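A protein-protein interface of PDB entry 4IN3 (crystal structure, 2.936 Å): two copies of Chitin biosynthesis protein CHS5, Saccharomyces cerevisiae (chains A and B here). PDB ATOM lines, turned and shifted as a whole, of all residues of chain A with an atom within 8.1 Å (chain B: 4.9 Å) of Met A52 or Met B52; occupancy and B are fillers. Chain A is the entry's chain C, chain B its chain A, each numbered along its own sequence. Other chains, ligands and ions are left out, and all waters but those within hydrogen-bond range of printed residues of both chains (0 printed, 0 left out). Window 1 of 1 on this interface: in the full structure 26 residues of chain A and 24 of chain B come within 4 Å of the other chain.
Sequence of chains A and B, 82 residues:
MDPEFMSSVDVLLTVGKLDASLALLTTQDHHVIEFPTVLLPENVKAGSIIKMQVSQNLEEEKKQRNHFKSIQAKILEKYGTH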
ATOM      1  N   SER A   8      29.752  16.026  -8.324  1.00  0.00           N
ATOM      2  CA  SER A   8      29.724  15.007  -7.288  1.00  0.00           C
ATOM      3  C   SER A   8      28.277  14.703  -6.920  1.00  0.00           C
ATOM      4  O   SER A   8      27.542  15.579  -6.450  1.00  0.00           O
ATOM      5  CB  SER A   8      30.474  15.478  -6.042  1.00  0.00           C
ATOM      6  OG  SER A   8      29.678  16.362  -5.266  1.00  0.00           O
ATOM      7  N   VAL A   9      27.862  13.464  -7.147  1.00  0.00           N
ATOM      8  CA  VAL A   9      26.518  13.054  -6.782  1.00  0.00           C
ATOM      9  C   VAL A   9      26.523  12.419  -5.401  1.00  0.00           C
ATOM     10  O   VAL A   9      27.196  11.413  -5.165  1.00  0.00           O
ATOM     11  CB  VAL A   9      25.930  12.072  -7.796  1.00  0.00           C
ATOM     12  CG1 VAL A   9      24.464  11.793  -7.465  1.00  0.00           C
ATOM     13  CG2 VAL A   9      26.060  12.637  -9.200  1.00  0.00           C
ATOM     14  N   ASP A  10      25.773  13.017  -4.484  1.00  0.00           N
ATOM     15  CA  ASP A  10      25.667  12.482  -3.136  1.00  0.00           C
ATOM     16  C   ASP A  10      24.357  11.726  -2.964  1.00  0.00           C
ATOM     17  O   ASP A  10      23.277  12.310  -3.036  1.00  0.00           O
ATOM     18  CB  ASP A  10      25.777  13.603  -2.100  1.00  0.00           C
ATOM     19  CG  ASP A  10      27.154  14.242  -2.074  1.00  0.00           C
ATOM     20  OD1 ASP A  10      27.821  14.269  -3.131  1.00  0.00           O
ATOM     21  OD2 ASP A  10      27.571  14.713  -0.995  1.00  0.00           O
ATOM     22  N   VAL A  11      24.456  10.418  -2.756  1.00  0.00           N
ATOM     23  CA  VAL A  11      23.278   9.606  -2.496  1.00  0.00           C
ATOM     24  C   VAL A  11      23.296   9.149  -1.044  1.00  0.00           C
ATOM     25  O   VAL A  11      24.348   8.795  -0.513  1.00  0.00           O
ATOM     26  CB  VAL A  11      23.230   8.367  -3.406  1.00  0.00           C
ATOM     27  CG1 VAL A  11      21.812   7.797  -3.449  1.00  0.00           C
ATOM     28  CG2 VAL A  11      23.698   8.722  -4.805  1.00  0.00           C
ATOM     29  N   LEU A  12      22.136   9.168  -0.398  1.00  0.00           N
ATOM     30  CA  LEU A  12      22.021   8.641   0.955  1.00  0.00           C
ATOM     31  C   LEU A  12      21.172   7.376   0.908  1.00  0.00           C
ATOM     32  O   LEU A  12      20.011   7.411   0.496  1.00  0.00           O
ATOM     33  CB  LEU A  12      21.392   9.666   1.898  1.00  0.00           C
ATOM     34  CG  LEU A  12      21.666   9.417   3.382  1.00  0.00           C
ATOM     35  CD1 LEU A  12      22.970  10.088   3.803  1.00  0.00           C
ATOM     36  CD2 LEU A  12      20.498   9.894   4.234  1.00  0.00           C
ATOM     37  N   LEU A  13      21.752   6.254   1.320  1.00  0.00           N
ATOM     38  CA  LEU A  13      21.060   4.976   1.203  1.00  0.00           C
ATOM     39  C   LEU A  13      20.856   4.297   2.555  1.00  0.00           C
ATOM     40  O   LEU A  13      21.639   4.501   3.485  1.00  0.00           O
ATOM     41  CB  LEU A  13      21.814   4.043   0.251  1.00  0.00           C
ATOM     42  CG  LEU A  13      22.109   4.616  -1.138  1.00  0.00           C
ATOM     43  CD1 LEU A  13      23.580   4.992  -1.263  1.00  0.00           C
ATOM     44  CD2 LEU A  13      21.702   3.644  -2.233  1.00  0.00           C
ATOM     45  N   LEU A  25      20.178  -1.822  -0.964  1.00  0.00           N
ATOM     46  CA  LEU A  25      20.198  -0.439  -0.512  1.00  0.00           C
ATOM     47  C   LEU A  25      18.934   0.267  -0.984  1.00  0.00           C
ATOM     48  O   LEU A  25      18.371  -0.082  -2.025  1.00  0.00           O
ATOM     49  CB  LEU A  25      21.451   0.269  -1.032  1.00  0.00           C
ATOM     50  CG  LEU A  25      22.765  -0.500  -0.849  1.00  0.00           C
ATOM     51  CD1 LEU A  25      23.927   0.244  -1.499  1.00  0.00           C
ATOM     52  CD2 LEU A  25      23.052  -0.759   0.622  1.00  0.00           C
ATOM     53  N   THR A  27      17.093   4.176  -1.484  1.00  0.00           N
ATOM     54  CA  THR A  27      17.072   5.636  -1.456  1.00  0.00           C
ATOM     55  C   THR A  27      15.768   6.143  -0.851  1.00  0.00           C
ATOM     56  O   THR A  27      14.857   5.362  -0.565  1.00  0.00           O
ATOM     57  CB  THR A  27      17.230   6.241  -2.866  1.00  0.00           C
ATOM     58  OG1 THR A  27      16.124   5.846  -3.686  1.00  0.00           O
ATOM     59  CG2 THR A  27      18.528   5.787  -3.514  1.00  0.00           C
ATOM     60  N   ILE A  33      18.950  -0.675  -4.807  1.00  0.00           N
ATOM     61  CA  ILE A  33      20.176  -1.112  -5.460  1.00  0.00           C
ATOM     62  C   ILE A  33      20.663  -2.441  -4.897  1.00  0.00           C
ATOM     63  O   ILE A  33      20.627  -2.662  -3.687  1.00  0.00           O
ATOM     64  CB  ILE A  33      21.301  -0.062  -5.333  1.00  0.00           C
ATOM     65  CG1 ILE A  33      20.762   1.341  -5.609  1.00  0.00           C
ATOM     66  CG2 ILE A  33      22.454  -0.379  -6.285  1.00  0.00           C
ATOM     67  CD1 ILE A  33      21.836   2.408  -5.625  1.00  0.00           C
ATOM     68  N   PHE A  35      23.813  -4.329  -4.146  1.00  0.00           N
ATOM     69  CA  PHE A  35      25.220  -4.006  -3.980  1.00  0.00           C
ATOM     70  C   PHE A  35      25.978  -5.214  -3.443  1.00  0.00           C
ATOM     71  O   PHE A  35      25.374  -6.125  -2.887  1.00  0.00           O
ATOM     72  CB  PHE A  35      25.361  -2.832  -3.011  1.00  0.00           C
ATOM     73  CG  PHE A  35      26.384  -1.813  -3.433  1.00  0.00           C
ATOM     74  CD1 PHE A  35      26.300  -1.198  -4.672  1.00  0.00           C
ATOM     75  CD2 PHE A  35      27.421  -1.456  -2.583  1.00  0.00           C
ATOM     76  CE1 PHE A  35      27.238  -0.254  -5.061  1.00  0.00           C
ATOM     77  CE2 PHE A  35      28.361  -0.515  -2.966  1.00  0.00           C
ATOM     78  CZ  PHE A  35      28.268   0.087  -4.207  1.00  0.00           C
ATOM     79  N   PRO A  36      27.306  -5.247  -3.650  1.00  0.00           N
ATOM     80  CA  PRO A  36      28.131  -6.238  -2.947  1.00  0.00           C
ATOM     81  C   PRO A  36      28.533  -5.697  -1.573  1.00  0.00           C
ATOM     82  O   PRO A  36      28.754  -4.493  -1.431  1.00  0.00           O
ATOM     83  CB  PRO A  36      29.358  -6.381  -3.851  1.00  0.00           C
ATOM     84  CG  PRO A  36      29.467  -5.062  -4.535  1.00  0.00           C
ATOM     85  CD  PRO A  36      28.056  -4.546  -4.707  1.00  0.00           C
ATOM     86  N   LEU A  39      32.111  -3.853  -0.847  1.00  0.00           N
ATOM     87  CA  LEU A  39      32.294  -2.445  -1.199  1.00  0.00           C
ATOM     88  C   LEU A  39      31.672  -1.545  -0.132  1.00  0.00           C
ATOM     89  O   LEU A  39      31.570  -0.331  -0.309  1.00  0.00           O
ATOM     90  CB  LEU A  39      31.705  -2.129  -2.578  1.00  0.00           C
ATOM     91  CG  LEU A  39      32.624  -2.291  -3.794  1.00  0.00           C
ATOM     92  CD1 LEU A  39      32.970  -3.749  -4.041  1.00  0.00           C
ATOM     93  CD2 LEU A  39      31.985  -1.675  -5.031  1.00  0.00           C
ATOM     94  N   LEU A  40      31.262  -2.155   0.976  1.00  0.00           N
ATOM     95  CA  LEU A  40      30.682  -1.433   2.099  1.00  0.00           C
ATOM     96  C   LEU A  40      31.600  -1.553   3.311  1.00  0.00           C
ATOM     97  O   LEU A  40      32.298  -2.557   3.460  1.00  0.00           O
ATOM     98  CB  LEU A  40      29.300  -1.999   2.431  1.00  0.00           C
ATOM     99  CG  LEU A  40      28.271  -1.937   1.300  1.00  0.00           C
ATOM    100  CD1 LEU A  40      26.954  -2.562   1.739  1.00  0.00           C
ATOM    101  CD2 LEU A  40      28.066  -0.497   0.859  1.00  0.00           C
ATOM    102  N   ILE A  49      22.832   3.627   7.898  1.00  0.00           N
ATOM    103  CA  ILE A  49      22.725   4.635   6.851  1.00  0.00           C
ATOM    104  C   ILE A  49      24.086   4.880   6.209  1.00  0.00           C
ATOM    105  O   ILE A  49      25.046   5.240   6.894  1.00  0.00           O
ATOM    106  CB  ILE A  49      22.182   5.967   7.397  1.00  0.00           C
ATOM    107  CG1 ILE A  49      21.142   5.720   8.493  1.00  0.00           C
ATOM    108  CG2 ILE A  49      21.607   6.805   6.264  1.00  0.00           C
ATOM    109  CD1 ILE A  49      19.883   5.019   8.019  1.00  0.00           C
ATOM    110  N   ILE A  50      24.175   4.678   4.896  1.00  0.00           N
ATOM    111  CA  ILE A  50      25.426   4.924   4.182  1.00  0.00           C
ATOM    112  C   ILE A  50      25.308   6.112   3.230  1.00  0.00           C
ATOM    113  O   ILE A  50      24.208   6.508   2.843  1.00  0.00           O
ATOM    114  CB  ILE A  50      25.908   3.678   3.399  1.00  0.00           C
ATOM    115  CG1 ILE A  50      25.089   3.484   2.122  1.00  0.00           C
ATOM    116  CG2 ILE A  50      25.859   2.437   4.278  1.00  0.00           C
ATOM    117  CD1 ILE A  50      25.558   2.315   1.276  1.00  0.00           C
ATOM    118  N   LYS A  51      26.451   6.672   2.851  1.00  0.00           N
ATOM    119  CA  LYS A  51      26.481   7.815   1.947  1.00  0.00           C
ATOM    120  C   LYS A  51      27.410   7.536   0.767  1.00  0.00           C
ATOM    121  O   LYS A  51      28.632   7.515   0.921  1.00  0.00           O
ATOM    122  CB  LYS A  51      26.940   9.063   2.703  1.00  0.00           C
ATOM    123  CG  LYS A  51      27.249  10.272   1.834  1.00  0.00           C
ATOM    124  CD  LYS A  51      27.877  11.373   2.680  1.00  0.00           C
ATOM    125  CE  LYS A  51      29.001  12.084   1.938  1.00  0.00           C
ATOM    126  NZ  LYS A  51      29.959  12.727   2.887  1.00  0.00           N
ATOM    127  N   MET A  52      26.833   7.308  -0.407  1.00  0.00           N
ATOM    128  CA  MET A  52      27.631   7.066  -1.603  1.00  0.00           C
ATOM    129  C   MET A  52      27.962   8.370  -2.332  1.00  0.00           C
ATOM    130  O   MET A  52      27.066   9.138  -2.685  1.00  0.00           O
ATOM    131  CB  MET A  52      26.935   6.066  -2.528  1.00  0.00           C
ATOM    132  CG  MET A  52      27.457   4.645  -2.375  1.00  0.00           C
ATOM    133  SD  MET A  52      26.412   3.414  -3.172  1.00  0.00           S
ATOM    134  CE  MET A  52      25.860   4.336  -4.602  1.00  0.00           C
ATOM    135  N   GLN A  53      29.254   8.603  -2.551  1.00  0.00           N
ATOM    136  CA  GLN A  53      29.741   9.849  -3.135  1.00  0.00           C
ATOM    137  C   GLN A  53      30.373   9.590  -4.496  1.00  0.00           C
ATOM    138  O   GLN A  53      31.484   9.069  -4.583  1.00  0.00           O
ATOM    139  CB  GLN A  53      30.763  10.487  -2.194  1.00  0.00           C
ATOM    140  CG  GLN A  53      30.976  11.971  -2.393  1.00  0.00           C
ATOM    141  CD  GLN A  53      31.523  12.646  -1.151  1.00  0.00           C
ATOM    142  OE1 GLN A  53      31.760  12.000  -0.127  1.00  0.00           O
ATOM    143  NE2 GLN A  53      31.718  13.957  -1.230  1.00  0.00           N
ATOM    144  N   VAL A  54      29.673   9.977  -5.558  1.00  0.00           N
ATOM    145  CA  VAL A  54      30.058   9.579  -6.911  1.00  0.00           C
ATOM    146  C   VAL A  54      30.675  10.706  -7.731  1.00  0.00           C
ATOM    147  O   VAL A  54      30.077  11.764  -7.902  1.00  0.00           O
ATOM    148  CB  VAL A  54      28.854   9.022  -7.696  1.00  0.00           C
ATOM    149  CG1 VAL A  54      29.308   8.398  -9.004  1.00  0.00           C
ATOM    150  CG2 VAL A  54      28.082   8.006  -6.857  1.00  0.00           C
ATOM    151  N   SER A  55      31.874  10.469  -8.246  1.00  0.00           N
ATOM    152  CA  SER A  55      32.549  11.453  -9.079  1.00  0.00           C
ATOM    153  C   SER A  55      33.109  10.810 -10.345  1.00  0.00           C
ATOM    154  O   SER A  55      33.497   9.643 -10.336  1.00  0.00           O
ATOM    155  CB  SER A  55      33.656  12.152  -8.285  1.00  0.00           C
ATOM    156  OG  SER A  55      34.214  11.289  -7.312  1.00  0.00           O
ATOM    157  N   GLN A  56      33.132  11.568 -11.436  1.00  0.00           N
ATOM    158  CA  GLN A  56      33.724  11.095 -12.681  1.00  0.00           C
ATOM    159  C   GLN A  56      35.238  11.233 -12.559  1.00  0.00           C
ATOM    160  O   GLN A  56      35.733  12.075 -11.804  1.00  0.00           O
ATOM    161  CB  GLN A  56      33.211  11.934 -13.853  1.00  0.00           C
ATOM    162  CG  GLN A  56      33.386  11.319 -15.239  1.00  0.00           C
ATOM    163  CD  GLN A  56      32.775  12.185 -16.336  1.00  0.00           C
ATOM    164  OE1 GLN A  56      32.425  13.344 -16.102  1.00  0.00           O
ATOM    165  NE2 GLN A  56      32.642  11.625 -17.535  1.00  0.00           N
ATOM    166  N   VAL B   9      35.211   3.592   2.031  1.00  0.00           N
ATOM    167  CA  VAL B   9      35.592   2.656   0.976  1.00  0.00           C
ATOM    168  C   VAL B   9      35.616   3.333  -0.394  1.00  0.00           C
ATOM    169  O   VAL B   9      34.579   3.760  -0.902  1.00  0.00           O
ATOM    170  CB  VAL B   9      34.637   1.446   0.926  1.00  0.00           C
ATOM    171  CG1 VAL B   9      34.982   0.543  -0.250  1.00  0.00           C
ATOM    172  CG2 VAL B   9      34.689   0.672   2.236  1.00  0.00           C
ATOM    173  N   ASP B  10      36.801   3.425  -0.991  1.00  0.00           N
ATOM    174  CA  ASP B  10      36.952   4.055  -2.300  1.00  0.00           C
ATOM    175  C   ASP B  10      37.055   3.020  -3.415  1.00  0.00           C
ATOM    176  O   ASP B  10      37.935   2.159  -3.400  1.00  0.00           O
ATOM    177  CB  ASP B  10      38.180   4.969  -2.327  1.00  0.00           C
ATOM    178  CG  ASP B  10      38.055   6.147  -1.380  1.00  0.00           C
ATOM    179  OD1 ASP B  10      37.377   7.132  -1.744  1.00  0.00           O
ATOM    180  OD2 ASP B  10      38.641   6.095  -0.277  1.00  0.00           O
ATOM    181  N   VAL B  11      36.148   3.105  -4.383  1.00  0.00           N
ATOM    182  CA  VAL B  11      36.158   2.175  -5.509  1.00  0.00           C
ATOM    183  C   VAL B  11      36.206   2.908  -6.844  1.00  0.00           C
ATOM    184  O   VAL B  11      35.694   4.017  -6.973  1.00  0.00           O
ATOM    185  CB  VAL B  11      34.912   1.269  -5.516  1.00  0.00           C
ATOM    186  CG1 VAL B  11      34.894   0.398  -6.769  1.00  0.00           C
ATOM    187  CG2 VAL B  11      34.865   0.403  -4.268  1.00  0.00           C
ATOM    188  N   LEU B  13      34.977   2.334 -10.810  1.00  0.00           N
ATOM    189  CA  LEU B  13      34.129   1.489 -11.641  1.00  0.00           C
ATOM    190  C   LEU B  13      34.098   1.997 -13.078  1.00  0.00           C
ATOM    191  O   LEU B  13      34.272   3.194 -13.334  1.00  0.00           O
ATOM    192  CB  LEU B  13      32.709   1.395 -11.068  1.00  0.00           C
ATOM    193  CG  LEU B  13      32.565   0.772  -9.676  1.00  0.00           C
ATOM    194  CD1 LEU B  13      32.555   1.842  -8.592  1.00  0.00           C
ATOM    195  CD2 LEU B  13      31.314  -0.102  -9.592  1.00  0.00           C
ATOM    196  N   LEU B  25      28.018  -1.633 -14.176  1.00  0.00           N
ATOM    197  CA  LEU B  25      29.345  -1.141 -13.838  1.00  0.00           C
ATOM    198  C   LEU B  25      30.259  -2.318 -13.518  1.00  0.00           C
ATOM    199  O   LEU B  25      29.823  -3.310 -12.934  1.00  0.00           O
ATOM    200  CB  LEU B  25      29.267  -0.179 -12.651  1.00  0.00           C
ATOM    201  CG  LEU B  25      28.181   0.901 -12.716  1.00  0.00           C
ATOM    202  CD1 LEU B  25      28.077   1.641 -11.388  1.00  0.00           C
ATOM    203  CD2 LEU B  25      28.434   1.884 -13.852  1.00  0.00           C
ATOM    204  N   PHE B  35      23.101  -0.472 -11.676  1.00  0.00           N
ATOM    205  CA  PHE B  35      23.048   0.824 -11.009  1.00  0.00           C
ATOM    206  C   PHE B  35      22.107   1.798 -11.714  1.00  0.00           C
ATOM    207  O   PHE B  35      22.084   1.854 -12.938  1.00  0.00           O
ATOM    208  CB  PHE B  35      24.457   1.409 -10.932  1.00  0.00           C
ATOM    209  CG  PHE B  35      24.618   2.482  -9.897  1.00  0.00           C
ATOM    210  CD1 PHE B  35      24.694   2.157  -8.554  1.00  0.00           C
ATOM    211  CD2 PHE B  35      24.711   3.816 -10.265  1.00  0.00           C
ATOM    212  CE1 PHE B  35      24.848   3.140  -7.597  1.00  0.00           C
ATOM    213  CE2 PHE B  35      24.867   4.806  -9.310  1.00  0.00           C
ATOM    214  CZ  PHE B  35      24.936   4.468  -7.972  1.00  0.00           C
ATOM    215  N   ILE B  50      34.215   6.097 -13.121  1.00  0.00           N
ATOM    216  CA  ILE B  50      33.669   6.838 -11.991  1.00  0.00           C
ATOM    217  C   ILE B  50      34.231   6.362 -10.657  1.00  0.00           C
ATOM    218  O   ILE B  50      34.545   5.182 -10.490  1.00  0.00           O
ATOM    219  CB  ILE B  50      32.136   6.735 -11.941  1.00  0.00           C
ATOM    220  CG1 ILE B  50      31.690   5.272 -12.015  1.00  0.00           C
ATOM    221  CG2 ILE B  50      31.512   7.527 -13.070  1.00  0.00           C
ATOM    222  CD1 ILE B  50      30.187   5.082 -12.102  1.00  0.00           C
ATOM    223  N   LYS B  51      34.353   7.285  -9.706  1.00  0.00           N
ATOM    224  CA  LYS B  51      34.800   6.943  -8.360  1.00  0.00           C
ATOM    225  C   LYS B  51      33.630   6.946  -7.383  1.00  0.00           C
ATOM    226  O   LYS B  51      32.882   7.923  -7.289  1.00  0.00           O
ATOM    227  CB  LYS B  51      35.886   7.904  -7.869  1.00  0.00           C
ATOM    228  CG  LYS B  51      36.231   7.733  -6.386  1.00  0.00           C
ATOM    229  CD  LYS B  51      37.255   8.763  -5.917  1.00  0.00           C
ATOM    230  CE  LYS B  51      38.666   8.185  -5.897  1.00  0.00           C
ATOM    231  NZ  LYS B  51      39.685   9.226  -5.561  1.00  0.00           N
ATOM    232  N   MET B  52      33.474   5.844  -6.661  1.00  0.00           N
ATOM    233  CA  MET B  52      32.433   5.736  -5.655  1.00  0.00           C
ATOM    234  C   MET B  52      33.064   5.730  -4.266  1.00  0.00           C
ATOM    235  O   MET B  52      33.839   4.831  -3.922  1.00  0.00           O
ATOM    236  CB  MET B  52      31.599   4.474  -5.874  1.00  0.00           C
ATOM    237  CG  MET B  52      30.330   4.427  -5.042  1.00  0.00           C
ATOM    238  SD  MET B  52      29.234   3.095  -5.570  1.00  0.00           S
ATOM    239  CE  MET B  52      29.119   3.429  -7.331  1.00  0.00           C
ATOM    240  N   GLN B  53      32.738   6.753  -3.484  1.00  0.00           N
ATOM    241  CA  GLN B  53      33.262   6.903  -2.136  1.00  0.00           C
ATOM    242  C   GLN B  53      32.155   6.570  -1.147  1.00  0.00           C
ATOM    243  O   GLN B  53      31.296   7.402  -0.853  1.00  0.00           O
ATOM    244  CB  GLN B  53      33.765   8.332  -1.920  1.00  0.00           C
ATOM    245  CG  GLN B  53      34.985   8.674  -2.760  1.00  0.00           C
ATOM    246  CD  GLN B  53      35.433  10.114  -2.594  1.00  0.00           C
ATOM    247  OE1 GLN B  53      34.637  10.989  -2.242  1.00  0.00           O
ATOM    248  NE2 GLN B  53      36.710  10.369  -2.850  1.00  0.00           N
ATOM    249  N   VAL B  54      32.176   5.342  -0.643  1.00  0.00           N
ATOM    250  CA  VAL B  54      31.128   4.864   0.245  1.00  0.00           C
ATOM    251  C   VAL B  54      31.504   5.117   1.698  1.00  0.00           C
ATOM    252  O   VAL B  54      32.468   4.544   2.212  1.00  0.00           O
ATOM    253  CB  VAL B  54      30.865   3.365   0.045  1.00  0.00           C
ATOM    254  CG1 VAL B  54      29.554   2.967   0.700  1.00  0.00           C
ATOM    255  CG2 VAL B  54      30.837   3.032  -1.440  1.00  0.00           C
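Of chain B, only Phe B35, Met B52, Gln B53 and Val B54 come within 4 Å of Met A52.
Printed residues of chain B within 4 Å of Gln A53: Lys B51 (3.3 Å), Met B52 (3.6 Å) and Gln B53 (2.9 Å).
Printed residues of chain A within 4 Å of Val B11: Leu A39 (3.5 Å).
Leu B25 touches none of the printed residues of chain A.
The nearest residue of chain A that does not touch Met B52 is Val A54 (4.6 Å).
Hydrophobic or aromatic side chains of chain A that line the printed part of chain B: Ile A33, Phe A35, Leu A39, Leu A40, Met A52 and Val A54.
Along chain A the printed residues that touch a printed residue of chain B span positions 33 to 55.
Hydrophobic or aromatic side chains of chain B that line the printed part of chain A: Val B9, Val B11, Phe B35, Ile B50, Met B52 and Val B54.
Among the printed residues, no Asp or Glu carboxylate lies within 4 Å of a Lys or Arg side-chain nitrogen of the other chain.
The backbone carbonyl oxygen (O) of Val B9 is in hydrogen-bond range of the backbone NH (N) of Val B54 (2.9 Å).
NE2 of Gln B53 sits close to OD1 of Asp B10 (3.5 Å).
O of Val B11 lies within hydrogen-bond range of N of Met B52, at 2.9 Å.
N of Leu B13 is in hydrogen-bond range of O of Ile B50, 2.9 Å away.
O of Val A11 sits at hydrogen-bond distance from N of Met A52, 2.9 Å away.
The backbone NH (N) of Leu A25 sits at hydrogen-bond distance from the backbone carbonyl oxygen (O) of Ile A33 (2.9 Å).
Lys A51 touches Gln B53, and with the chains exchanged Gln A53 touches Lys B51.
Met A52 touches its own counterpart, Met B52.
Met A52 touches Gln B53, and with the chains exchanged Gln A53 touches Met B52.
Gln B53 touches its own counterpart, Gln A53.
The backbone carbonyl oxygen (O) of Ser A55 is in hydrogen-bond range of the backbone NH (N) of Lys B51, at 2.6 Å.
N of Gln B53 sits at hydrogen-bond distance from O of Gln A53 (2.9 Å).
The backbone carbonyl oxygen (O) of Gln B53 sits close to the backbone carbonyl oxygen (O) of Lys A51 (3.2 Å).
SD of Met A52 sits close to SD of Met B52.
The backbone carbonyl oxygen (O) of Lys B51 sits close to the backbone carbonyl oxygen (O) of Gln A53 (3.3 Å).
CD1 of Ile A33 touches CE1 of Phe B35 (3.7 Å).
O of Leu A39 touches CG2 of Val B54, 3.6 Å away.
Leu A40 touches Val B54.
Lys A51 touches Val B54.
Phe B35 touches Met A52 (CE1 to CE, 3.4 Å).
CA of Met A52 touches O of Gln B53, at 3.8 Å.
CG2 of Val B54 touches CG of Met A52, at 3.9 Å.
Gln A53 touches Met B52.
CA of Val A54 touches O of Lys B51, at 3.3 Å.
Ile B50 touches Ser A55 (CA to O, 3.3 Å).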
